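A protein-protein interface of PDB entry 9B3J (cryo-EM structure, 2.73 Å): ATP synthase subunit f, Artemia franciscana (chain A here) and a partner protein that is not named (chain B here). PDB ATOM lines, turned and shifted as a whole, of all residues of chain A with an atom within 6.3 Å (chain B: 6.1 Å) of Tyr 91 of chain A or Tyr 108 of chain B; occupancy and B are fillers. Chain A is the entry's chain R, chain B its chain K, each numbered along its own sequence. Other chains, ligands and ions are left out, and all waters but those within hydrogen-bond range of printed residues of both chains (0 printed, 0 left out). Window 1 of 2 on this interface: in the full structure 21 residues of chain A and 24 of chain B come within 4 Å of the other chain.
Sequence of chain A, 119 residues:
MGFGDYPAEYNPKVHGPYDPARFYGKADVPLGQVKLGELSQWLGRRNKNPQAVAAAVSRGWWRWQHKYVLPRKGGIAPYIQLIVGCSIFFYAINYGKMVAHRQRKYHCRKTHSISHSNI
O of Leu 102 of chain B sits at hydrogen-bond distance from N of Tyr 108 of chain B (3.3 Å).
N of Ile 107 of chain B lies within hydrogen-bond range of O of Leu 102 of chain B (3.1 Å).
Hydrophobic or aromatic side chains of chain B within 4 Å of the printed part of chain A: Ile 107 and Val 109.
Of the 13 printed residues of chain A, 3 touch a printed residue of chain B.
Among the printed residues, 7 pairs touch across the chains.
Tyr 108 of chain B touches just one residue of chain A: Tyr 91.
Of the printed residues of chain A, Ile 107 of chain B touches Tyr 91 (2.3 Å) and Tyr 95 (3.3 Å).
Printed residues of chain A within 4 Å of Val 109 of chain B: Tyr 91 (3.3 Å) and Met 98 (3.4 Å).
Tyr 108 of chain B touches Tyr 91 of chain A.
Tyr 95 of chain A touches Ile 107 of chain B (OH to CG2, 3.3 Å).
Met 98 of chain A touches Val 109 of chain B (O to CG2, 3.4 Å).
Glu 113 of chain B touches Met 98 of chain A.
OH of Tyr 91 of chain A lies close to O of Ile 107 of chain B, 2.3 Å away.
The side-chain carboxylate (OE2) of Glu 111 of chain B sits close to the backbone carbonyl oxygen (O) of Met 98 of chain A (3.2 Å).
The side-chain hydroxyl (OH) of Tyr 91 of chain A lies within hydrogen-bond range of the backbone NH (N) of Val 109 of chain B (3.3 Å).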
ATOM      1  N   CYS A  86      28.179 -16.734   5.622  1.00  0.00           N
ATOM      2  CA  CYS A  86      26.730 -16.600   5.514  1.00  0.00           C
ATOM      3  C   CYS A  86      26.126 -17.718   4.678  1.00  0.00           C
ATOM      4  O   CYS A  86      25.025 -18.187   4.975  1.00  0.00           O
ATOM      5  CB  CYS A  86      26.366 -15.246   4.913  1.00  0.00           C
ATOM      6  SG  CYS A  86      26.639 -13.857   6.016  1.00  0.00           S
ATOM      7  N   SER A  87      26.823 -18.159   3.630  1.00  0.00           N
ATOM      8  CA  SER A  87      26.293 -19.229   2.791  1.00  0.00           C
ATOM      9  C   SER A  87      26.320 -20.572   3.505  1.00  0.00           C
ATOM     10  O   SER A  87      25.405 -21.383   3.342  1.00  0.00           O
ATOM     11  CB  SER A  87      27.075 -19.304   1.490  1.00  0.00           C
ATOM     12  OG  SER A  87      26.577 -20.351   0.692  1.00  0.00           O
ATOM     13  N   ILE A  88      27.354 -20.826   4.307  1.00  0.00           N
ATOM     14  CA  ILE A  88      27.393 -22.042   5.112  1.00  0.00           C
ATOM     15  C   ILE A  88      26.307 -22.016   6.176  1.00  0.00           C
ATOM     16  O   ILE A  88      25.609 -23.018   6.395  1.00  0.00           O
ATOM     17  CB  ILE A  88      28.787 -22.215   5.735  1.00  0.00           C
ATOM     18  CG1 ILE A  88      29.796 -22.613   4.666  1.00  0.00           C
ATOM     19  CG2 ILE A  88      28.766 -23.230   6.861  1.00  0.00           C
ATOM     20  CD1 ILE A  88      31.200 -22.721   5.188  1.00  0.00           C
ATOM     21  N   PHE A  89      26.144 -20.872   6.859  1.00  0.00           N
ATOM     22  CA  PHE A  89      25.108 -20.769   7.880  1.00  0.00           C
ATOM     23  C   PHE A  89      23.714 -20.912   7.287  1.00  0.00           C
ATOM     24  O   PHE A  89      22.856 -21.594   7.858  1.00  0.00           O
ATOM     25  CB  PHE A  89      25.241 -19.442   8.608  1.00  0.00           C
ATOM     26  CG  PHE A  89      24.169 -19.199   9.611  1.00  0.00           C
ATOM     27  CD1 PHE A  89      24.078 -19.982  10.745  1.00  0.00           C
ATOM     28  CD2 PHE A  89      23.258 -18.177   9.432  1.00  0.00           C
ATOM     29  CE1 PHE A  89      23.094 -19.756  11.678  1.00  0.00           C
ATOM     30  CE2 PHE A  89      22.273 -17.945  10.364  1.00  0.00           C
ATOM     31  CZ  PHE A  89      22.189 -18.737  11.486  1.00  0.00           C
ATOM     32  N   PHE A  90      23.469 -20.301   6.135  1.00  0.00           N
ATOM     33  CA  PHE A  90      22.165 -20.441   5.516  1.00  0.00           C
ATOM     34  C   PHE A  90      21.968 -21.789   4.851  1.00  0.00           C
ATOM     35  O   PHE A  90      20.832 -22.131   4.517  1.00  0.00           O
ATOM     36  CB  PHE A  90      21.942 -19.328   4.502  1.00  0.00           C
ATOM     37  CG  PHE A  90      21.298 -18.118   5.082  1.00  0.00           C
ATOM     38  CD1 PHE A  90      21.961 -17.360   6.023  1.00  0.00           C
ATOM     39  CD2 PHE A  90      20.030 -17.744   4.696  1.00  0.00           C
ATOM     40  CE1 PHE A  90      21.375 -16.253   6.563  1.00  0.00           C
ATOM     41  CE2 PHE A  90      19.439 -16.637   5.235  1.00  0.00           C
ATOM     42  CZ  PHE A  90      20.113 -15.889   6.169  1.00  0.00           C
ATOM     43  N   TYR A  91      23.034 -22.549   4.616  1.00  0.00           N
ATOM     44  CA  TYR A  91      22.831 -23.933   4.212  1.00  0.00           C
ATOM     45  C   TYR A  91      22.473 -24.804   5.403  1.00  0.00           C
ATOM     46  O   TYR A  91      21.650 -25.714   5.281  1.00  0.00           O
ATOM     47  CB  TYR A  91      24.075 -24.473   3.519  1.00  0.00           C
ATOM     48  CG  TYR A  91      23.988 -25.933   3.172  1.00  0.00           C
ATOM     49  CD1 TYR A  91      23.263 -26.352   2.077  1.00  0.00           C
ATOM     50  CD2 TYR A  91      24.642 -26.888   3.933  1.00  0.00           C
ATOM     51  CE1 TYR A  91      23.181 -27.674   1.751  1.00  0.00           C
ATOM     52  CE2 TYR A  91      24.561 -28.215   3.616  1.00  0.00           C
ATOM     53  CZ  TYR A  91      23.825 -28.599   2.523  1.00  0.00           C
ATOM     54  OH  TYR A  91      23.726 -29.921   2.183  1.00  0.00           O
ATOM     55  N   ALA A  92      23.092 -24.551   6.557  1.00  0.00           N
ATOM     56  CA  ALA A  92      22.743 -25.314   7.749  1.00  0.00           C
ATOM     57  C   ALA A  92      21.335 -24.992   8.220  1.00  0.00           C
ATOM     58  O   ALA A  92      20.683 -25.836   8.842  1.00  0.00           O
ATOM     59  CB  ALA A  92      23.747 -25.049   8.866  1.00  0.00           C
ATOM     60  N   ILE A  93      20.859 -23.779   7.946  1.00  0.00           N
ATOM     61  CA  ILE A  93      19.465 -23.445   8.221  1.00  0.00           C
ATOM     62  C   ILE A  93      18.535 -24.236   7.307  1.00  0.00           C
ATOM     63  O   ILE A  93      17.531 -24.800   7.758  1.00  0.00           O
ATOM     64  CB  ILE A  93      19.256 -21.928   8.084  1.00  0.00           C
ATOM     65  CG1 ILE A  93      19.771 -21.212   9.322  1.00  0.00           C
ATOM     66  CG2 ILE A  93      17.812 -21.599   7.873  1.00  0.00           C
ATOM     67  CD1 ILE A  93      19.435 -19.750   9.340  1.00  0.00           C
ATOM     68  N   ASN A  94      18.871 -24.331   6.025  1.00  0.00           N
ATOM     69  CA  ASN A  94      18.055 -25.051   5.051  1.00  0.00           C
ATOM     70  C   ASN A  94      18.519 -26.480   4.882  1.00  0.00           C
ATOM     71  O   ASN A  94      18.516 -26.999   3.766  1.00  0.00           O
ATOM     72  CB  ASN A  94      18.077 -24.331   3.711  1.00  0.00           C
ATOM     73  CG  ASN A  94      17.654 -22.899   3.818  1.00  0.00           C
ATOM     74  OD1 ASN A  94      17.062 -22.496   4.808  1.00  0.00           O
ATOM     75  ND2 ASN A  94      17.949 -22.115   2.792  1.00  0.00           N
ATOM     76  N   TYR A  95      18.961 -27.109   5.973  1.00  0.00           N
ATOM     77  CA  TYR A  95      19.501 -28.465   5.918  1.00  0.00           C
ATOM     78  C   TYR A  95      18.478 -29.444   5.359  1.00  0.00           C
ATOM     79  O   TYR A  95      18.794 -30.250   4.476  1.00  0.00           O
ATOM     80  CB  TYR A  95      19.938 -28.887   7.318  1.00  0.00           C
ATOM     81  CG  TYR A  95      20.919 -30.028   7.386  1.00  0.00           C
ATOM     82  CD1 TYR A  95      20.489 -31.341   7.310  1.00  0.00           C
ATOM     83  CD2 TYR A  95      22.272 -29.790   7.570  1.00  0.00           C
ATOM     84  CE1 TYR A  95      21.378 -32.386   7.389  1.00  0.00           C
ATOM     85  CE2 TYR A  95      23.171 -30.825   7.652  1.00  0.00           C
ATOM     86  CZ  TYR A  95      22.718 -32.124   7.559  1.00  0.00           C
ATOM     87  OH  TYR A  95      23.606 -33.171   7.639  1.00  0.00           O
ATOM     88  N   GLY A  96      17.240 -29.369   5.843  1.00  0.00           N
ATOM     89  CA  GLY A  96      16.205 -30.268   5.354  1.00  0.00           C
ATOM     90  C   GLY A  96      15.806 -30.003   3.916  1.00  0.00           C
ATOM     91  O   GLY A  96      15.556 -30.938   3.148  1.00  0.00           O
ATOM     92  N   MET A  98      17.566 -28.995   1.465  1.00  0.00           N
ATOM     93  CA  MET A  98      18.557 -29.502   0.526  1.00  0.00           C
ATOM     94  C   MET A  98      18.771 -31.002   0.648  1.00  0.00           C
ATOM     95  O   MET A  98      19.070 -31.656  -0.356  1.00  0.00           O
ATOM     96  CB  MET A  98      19.896 -28.786   0.723  1.00  0.00           C
ATOM     97  CG  MET A  98      19.790 -27.275   0.787  1.00  0.00           C
ATOM     98  SD  MET A  98      19.188 -26.524  -0.726  1.00  0.00           S
ATOM     99  CE  MET A  98      19.072 -24.814  -0.216  1.00  0.00           C
ATOM    100  N   VAL A  99      18.625 -31.560   1.852  1.00  0.00           N
ATOM    101  CA  VAL A  99      18.764 -33.001   2.027  1.00  0.00           C
ATOM    102  C   VAL A  99      17.623 -33.733   1.334  1.00  0.00           C
ATOM    103  O   VAL A  99      17.831 -34.773   0.697  1.00  0.00           O
ATOM    104  CB  VAL A  99      18.856 -33.336   3.529  1.00  0.00           C
ATOM    105  CG1 VAL A  99      18.272 -34.707   3.844  1.00  0.00           C
ATOM    106  CG2 VAL A  99      20.306 -33.250   3.996  1.00  0.00           C
ATOM    107  N   LEU B  99      35.787 -32.103   2.324  1.00  0.00           N
ATOM    108  CA  LEU B  99      34.949 -31.909   1.146  1.00  0.00           C
ATOM    109  C   LEU B  99      34.563 -33.240   0.517  1.00  0.00           C
ATOM    110  O   LEU B  99      33.432 -33.406   0.039  1.00  0.00           O
ATOM    111  CB  LEU B  99      35.668 -31.030   0.130  1.00  0.00           C
ATOM    112  CG  LEU B  99      34.828 -30.623  -1.077  1.00  0.00           C
ATOM    113  CD1 LEU B  99      33.640 -29.798  -0.625  1.00  0.00           C
ATOM    114  CD2 LEU B  99      35.670 -29.861  -2.081  1.00  0.00           C
ATOM    115  N   LEU B 102      31.811 -34.695   2.789  1.00  0.00           N
ATOM    116  CA  LEU B 102      30.526 -34.043   2.571  1.00  0.00           C
ATOM    117  C   LEU B 102      29.896 -34.496   1.264  1.00  0.00           C
ATOM    118  O   LEU B 102      28.689 -34.753   1.209  1.00  0.00           O
ATOM    119  CB  LEU B 102      30.680 -32.527   2.579  1.00  0.00           C
ATOM    120  CG  LEU B 102      31.042 -31.870   3.902  1.00  0.00           C
ATOM    121  CD1 LEU B 102      30.947 -30.371   3.752  1.00  0.00           C
ATOM    122  CD2 LEU B 102      30.130 -32.366   4.998  1.00  0.00           C
ATOM    123  N   LEU B 103      30.689 -34.608   0.204  1.00  0.00           N
ATOM    124  CA  LEU B 103      30.134 -35.104  -1.044  1.00  0.00           C
ATOM    125  C   LEU B 103      29.944 -36.617  -1.050  1.00  0.00           C
ATOM    126  O   LEU B 103      29.257 -37.131  -1.935  1.00  0.00           O
ATOM    127  CB  LEU B 103      31.023 -34.686  -2.215  1.00  0.00           C
ATOM    128  CG  LEU B 103      31.190 -33.186  -2.454  1.00  0.00           C
ATOM    129  CD1 LEU B 103      32.199 -32.934  -3.553  1.00  0.00           C
ATOM    130  CD2 LEU B 103      29.870 -32.556  -2.812  1.00  0.00           C
ATOM    131  N   LYS B 105      28.845 -38.801   1.831  1.00  0.00           N
ATOM    132  CA  LYS B 105      27.601 -39.075   2.527  1.00  0.00           C
ATOM    133  C   LYS B 105      26.477 -38.135   2.121  1.00  0.00           C
ATOM    134  O   LYS B 105      25.404 -38.202   2.728  1.00  0.00           O
ATOM    135  CB  LYS B 105      27.815 -39.001   4.037  1.00  0.00           C
ATOM    136  CG  LYS B 105      28.416 -40.256   4.646  1.00  0.00           C
ATOM    137  CD  LYS B 105      28.060 -40.354   6.129  1.00  0.00           C
ATOM    138  CE  LYS B 105      28.467 -41.688   6.738  1.00  0.00           C
ATOM    139  NZ  LYS B 105      28.074 -41.779   8.169  1.00  0.00           N
ATOM    140  N   GLU B 106      26.710 -37.264   1.134  1.00  0.00           N
ATOM    141  CA  GLU B 106      25.717 -36.329   0.601  1.00  0.00           C
ATOM    142  C   GLU B 106      25.154 -35.409   1.674  1.00  0.00           C
ATOM    143  O   GLU B 106      23.988 -35.019   1.620  1.00  0.00           O
ATOM    144  CB  GLU B 106      24.586 -37.059  -0.119  1.00  0.00           C
ATOM    145  CG  GLU B 106      24.848 -37.260  -1.585  1.00  0.00           C
ATOM    146  CD  GLU B 106      23.768 -38.073  -2.249  1.00  0.00           C
ATOM    147  OE1 GLU B 106      23.118 -38.878  -1.551  1.00  0.00           O
ATOM    148  OE2 GLU B 106      23.567 -37.907  -3.469  1.00  0.00           O
ATOM    149  N   ILE B 107      25.973 -35.076   2.671  1.00  0.00           N
ATOM    150  CA  ILE B 107      25.618 -34.001   3.586  1.00  0.00           C
ATOM    151  C   ILE B 107      25.553 -32.684   2.832  1.00  0.00           C
ATOM    152  O   ILE B 107      24.613 -31.900   2.998  1.00  0.00           O
ATOM    153  CB  ILE B 107      26.619 -33.943   4.748  1.00  0.00           C
ATOM    154  CG1 ILE B 107      26.620 -35.270   5.497  1.00  0.00           C
ATOM    155  CG2 ILE B 107      26.276 -32.817   5.679  1.00  0.00           C
ATOM    156  CD1 ILE B 107      27.609 -35.311   6.623  1.00  0.00           C
ATOM    157  N   TYR B 108      26.540 -32.430   1.982  1.00  0.00           N
ATOM    158  CA  TYR B 108      26.489 -31.322   1.039  1.00  0.00           C
ATOM    159  C   TYR B 108      25.905 -31.855  -0.256  1.00  0.00           C
ATOM    160  O   TYR B 108      26.577 -32.579  -0.993  1.00  0.00           O
ATOM    161  CB  TYR B 108      27.876 -30.728   0.816  1.00  0.00           C
ATOM    162  CG  TYR B 108      27.883 -29.545  -0.121  1.00  0.00           C
ATOM    163  CD1 TYR B 108      27.657 -28.265   0.350  1.00  0.00           C
ATOM    164  CD2 TYR B 108      28.117 -29.708  -1.476  1.00  0.00           C
ATOM    165  CE1 TYR B 108      27.657 -27.189  -0.497  1.00  0.00           C
ATOM    166  CE2 TYR B 108      28.118 -28.638  -2.329  1.00  0.00           C
ATOM    167  CZ  TYR B 108      27.888 -27.383  -1.835  1.00  0.00           C
ATOM    168  OH  TYR B 108      27.893 -26.317  -2.696  1.00  0.00           O
ATOM    169  N   VAL B 109      24.668 -31.496  -0.541  1.00  0.00           N
ATOM    170  CA  VAL B 109      23.978 -31.991  -1.723  1.00  0.00           C
ATOM    171  C   VAL B 109      24.268 -31.064  -2.892  1.00  0.00           C
ATOM    172  O   VAL B 109      24.084 -29.847  -2.790  1.00  0.00           O
ATOM    173  CB  VAL B 109      22.469 -32.095  -1.471  1.00  0.00           C
ATOM    174  CG1 VAL B 109      21.803 -32.817  -2.616  1.00  0.00           C
ATOM    175  CG2 VAL B 109      22.216 -32.804  -0.169  1.00  0.00           C
ATOM    176  N   VAL B 110      24.708 -31.637  -4.009  1.00  0.00           N
ATOM    177  CA  VAL B 110      25.002 -30.849  -5.201  1.00  0.00           C
ATOM    178  C   VAL B 110      23.664 -30.497  -5.843  1.00  0.00           C
ATOM    179  O   VAL B 110      23.095 -31.278  -6.605  1.00  0.00           O
ATOM    180  CB  VAL B 110      25.919 -31.598  -6.166  1.00  0.00           C
ATOM    181  CG1 VAL B 110      26.194 -30.763  -7.401  1.00  0.00           C
ATOM    182  CG2 VAL B 110      27.212 -31.954  -5.469  1.00  0.00           C
ATOM    183  N   GLU B 111      23.155 -29.318  -5.524  1.00  0.00           N
ATOM    184  CA  GLU B 111      21.867 -28.860  -6.006  1.00  0.00           C
ATOM    185  C   GLU B 111      22.060 -27.858  -7.135  1.00  0.00           C
ATOM    186  O   GLU B 111      23.165 -27.662  -7.646  1.00  0.00           O
ATOM    187  CB  GLU B 111      21.057 -28.261  -4.857  1.00  0.00           C
ATOM    188  CG  GLU B 111      20.421 -29.289  -3.945  1.00  0.00           C
ATOM    189  CD  GLU B 111      19.058 -28.855  -3.451  1.00  0.00           C
ATOM    190  OE1 GLU B 111      18.666 -27.702  -3.726  1.00  0.00           O
ATOM    191  OE2 GLU B 111      18.374 -29.669  -2.799  1.00  0.00           O
ATOM    192  N   GLU B 113      22.050 -24.782  -6.831  1.00  0.00           N
ATOM    193  CA  GLU B 113      22.764 -23.619  -6.331  1.00  0.00           C
ATOM    194  C   GLU B 113      24.265 -23.830  -6.233  1.00  0.00           C
ATOM    195  O   GLU B 113      24.995 -22.852  -6.060  1.00  0.00           O
ATOM    196  CB  GLU B 113      22.214 -23.216  -4.961  1.00  0.00           C
ATOM    197  CG  GLU B 113      20.790 -22.704  -5.032  1.00  0.00           C
ATOM    198  CD  GLU B 113      20.239 -22.343  -3.678  1.00  0.00           C
ATOM    199  OE1 GLU B 113      20.959 -22.544  -2.684  1.00  0.00           O
ATOM    200  OE2 GLU B 113      19.093 -21.853  -3.603  1.00  0.00           O
ATOM    201  N   PHE B 114      24.741 -25.068  -6.334  1.00  0.00           N
ATOM    202  CA  PHE B 114      26.180 -25.299  -6.352  1.00  0.00           C
ATOM    203  C   PHE B 114      26.814 -24.716  -7.605  1.00  0.00           C
ATOM    204  O   PHE B 114      27.916 -24.163  -7.551  1.00  0.00           O
ATOM    205  CB  PHE B 114      26.469 -26.792  -6.245  1.00  0.00           C
ATOM    206  CG  PHE B 114      27.882 -27.162  -6.570  1.00  0.00           C
ATOM    207  CD1 PHE B 114      28.898 -26.903  -5.676  1.00  0.00           C
ATOM    208  CD2 PHE B 114      28.191 -27.786  -7.766  1.00  0.00           C
ATOM    209  CE1 PHE B 114      30.199 -27.249  -5.971  1.00  0.00           C
ATOM    210  CE2 PHE B 114      29.488 -28.132  -8.065  1.00  0.00           C
ATOM    211  CZ  PHE B 114      30.493 -27.862  -7.168  1.00  0.00           C
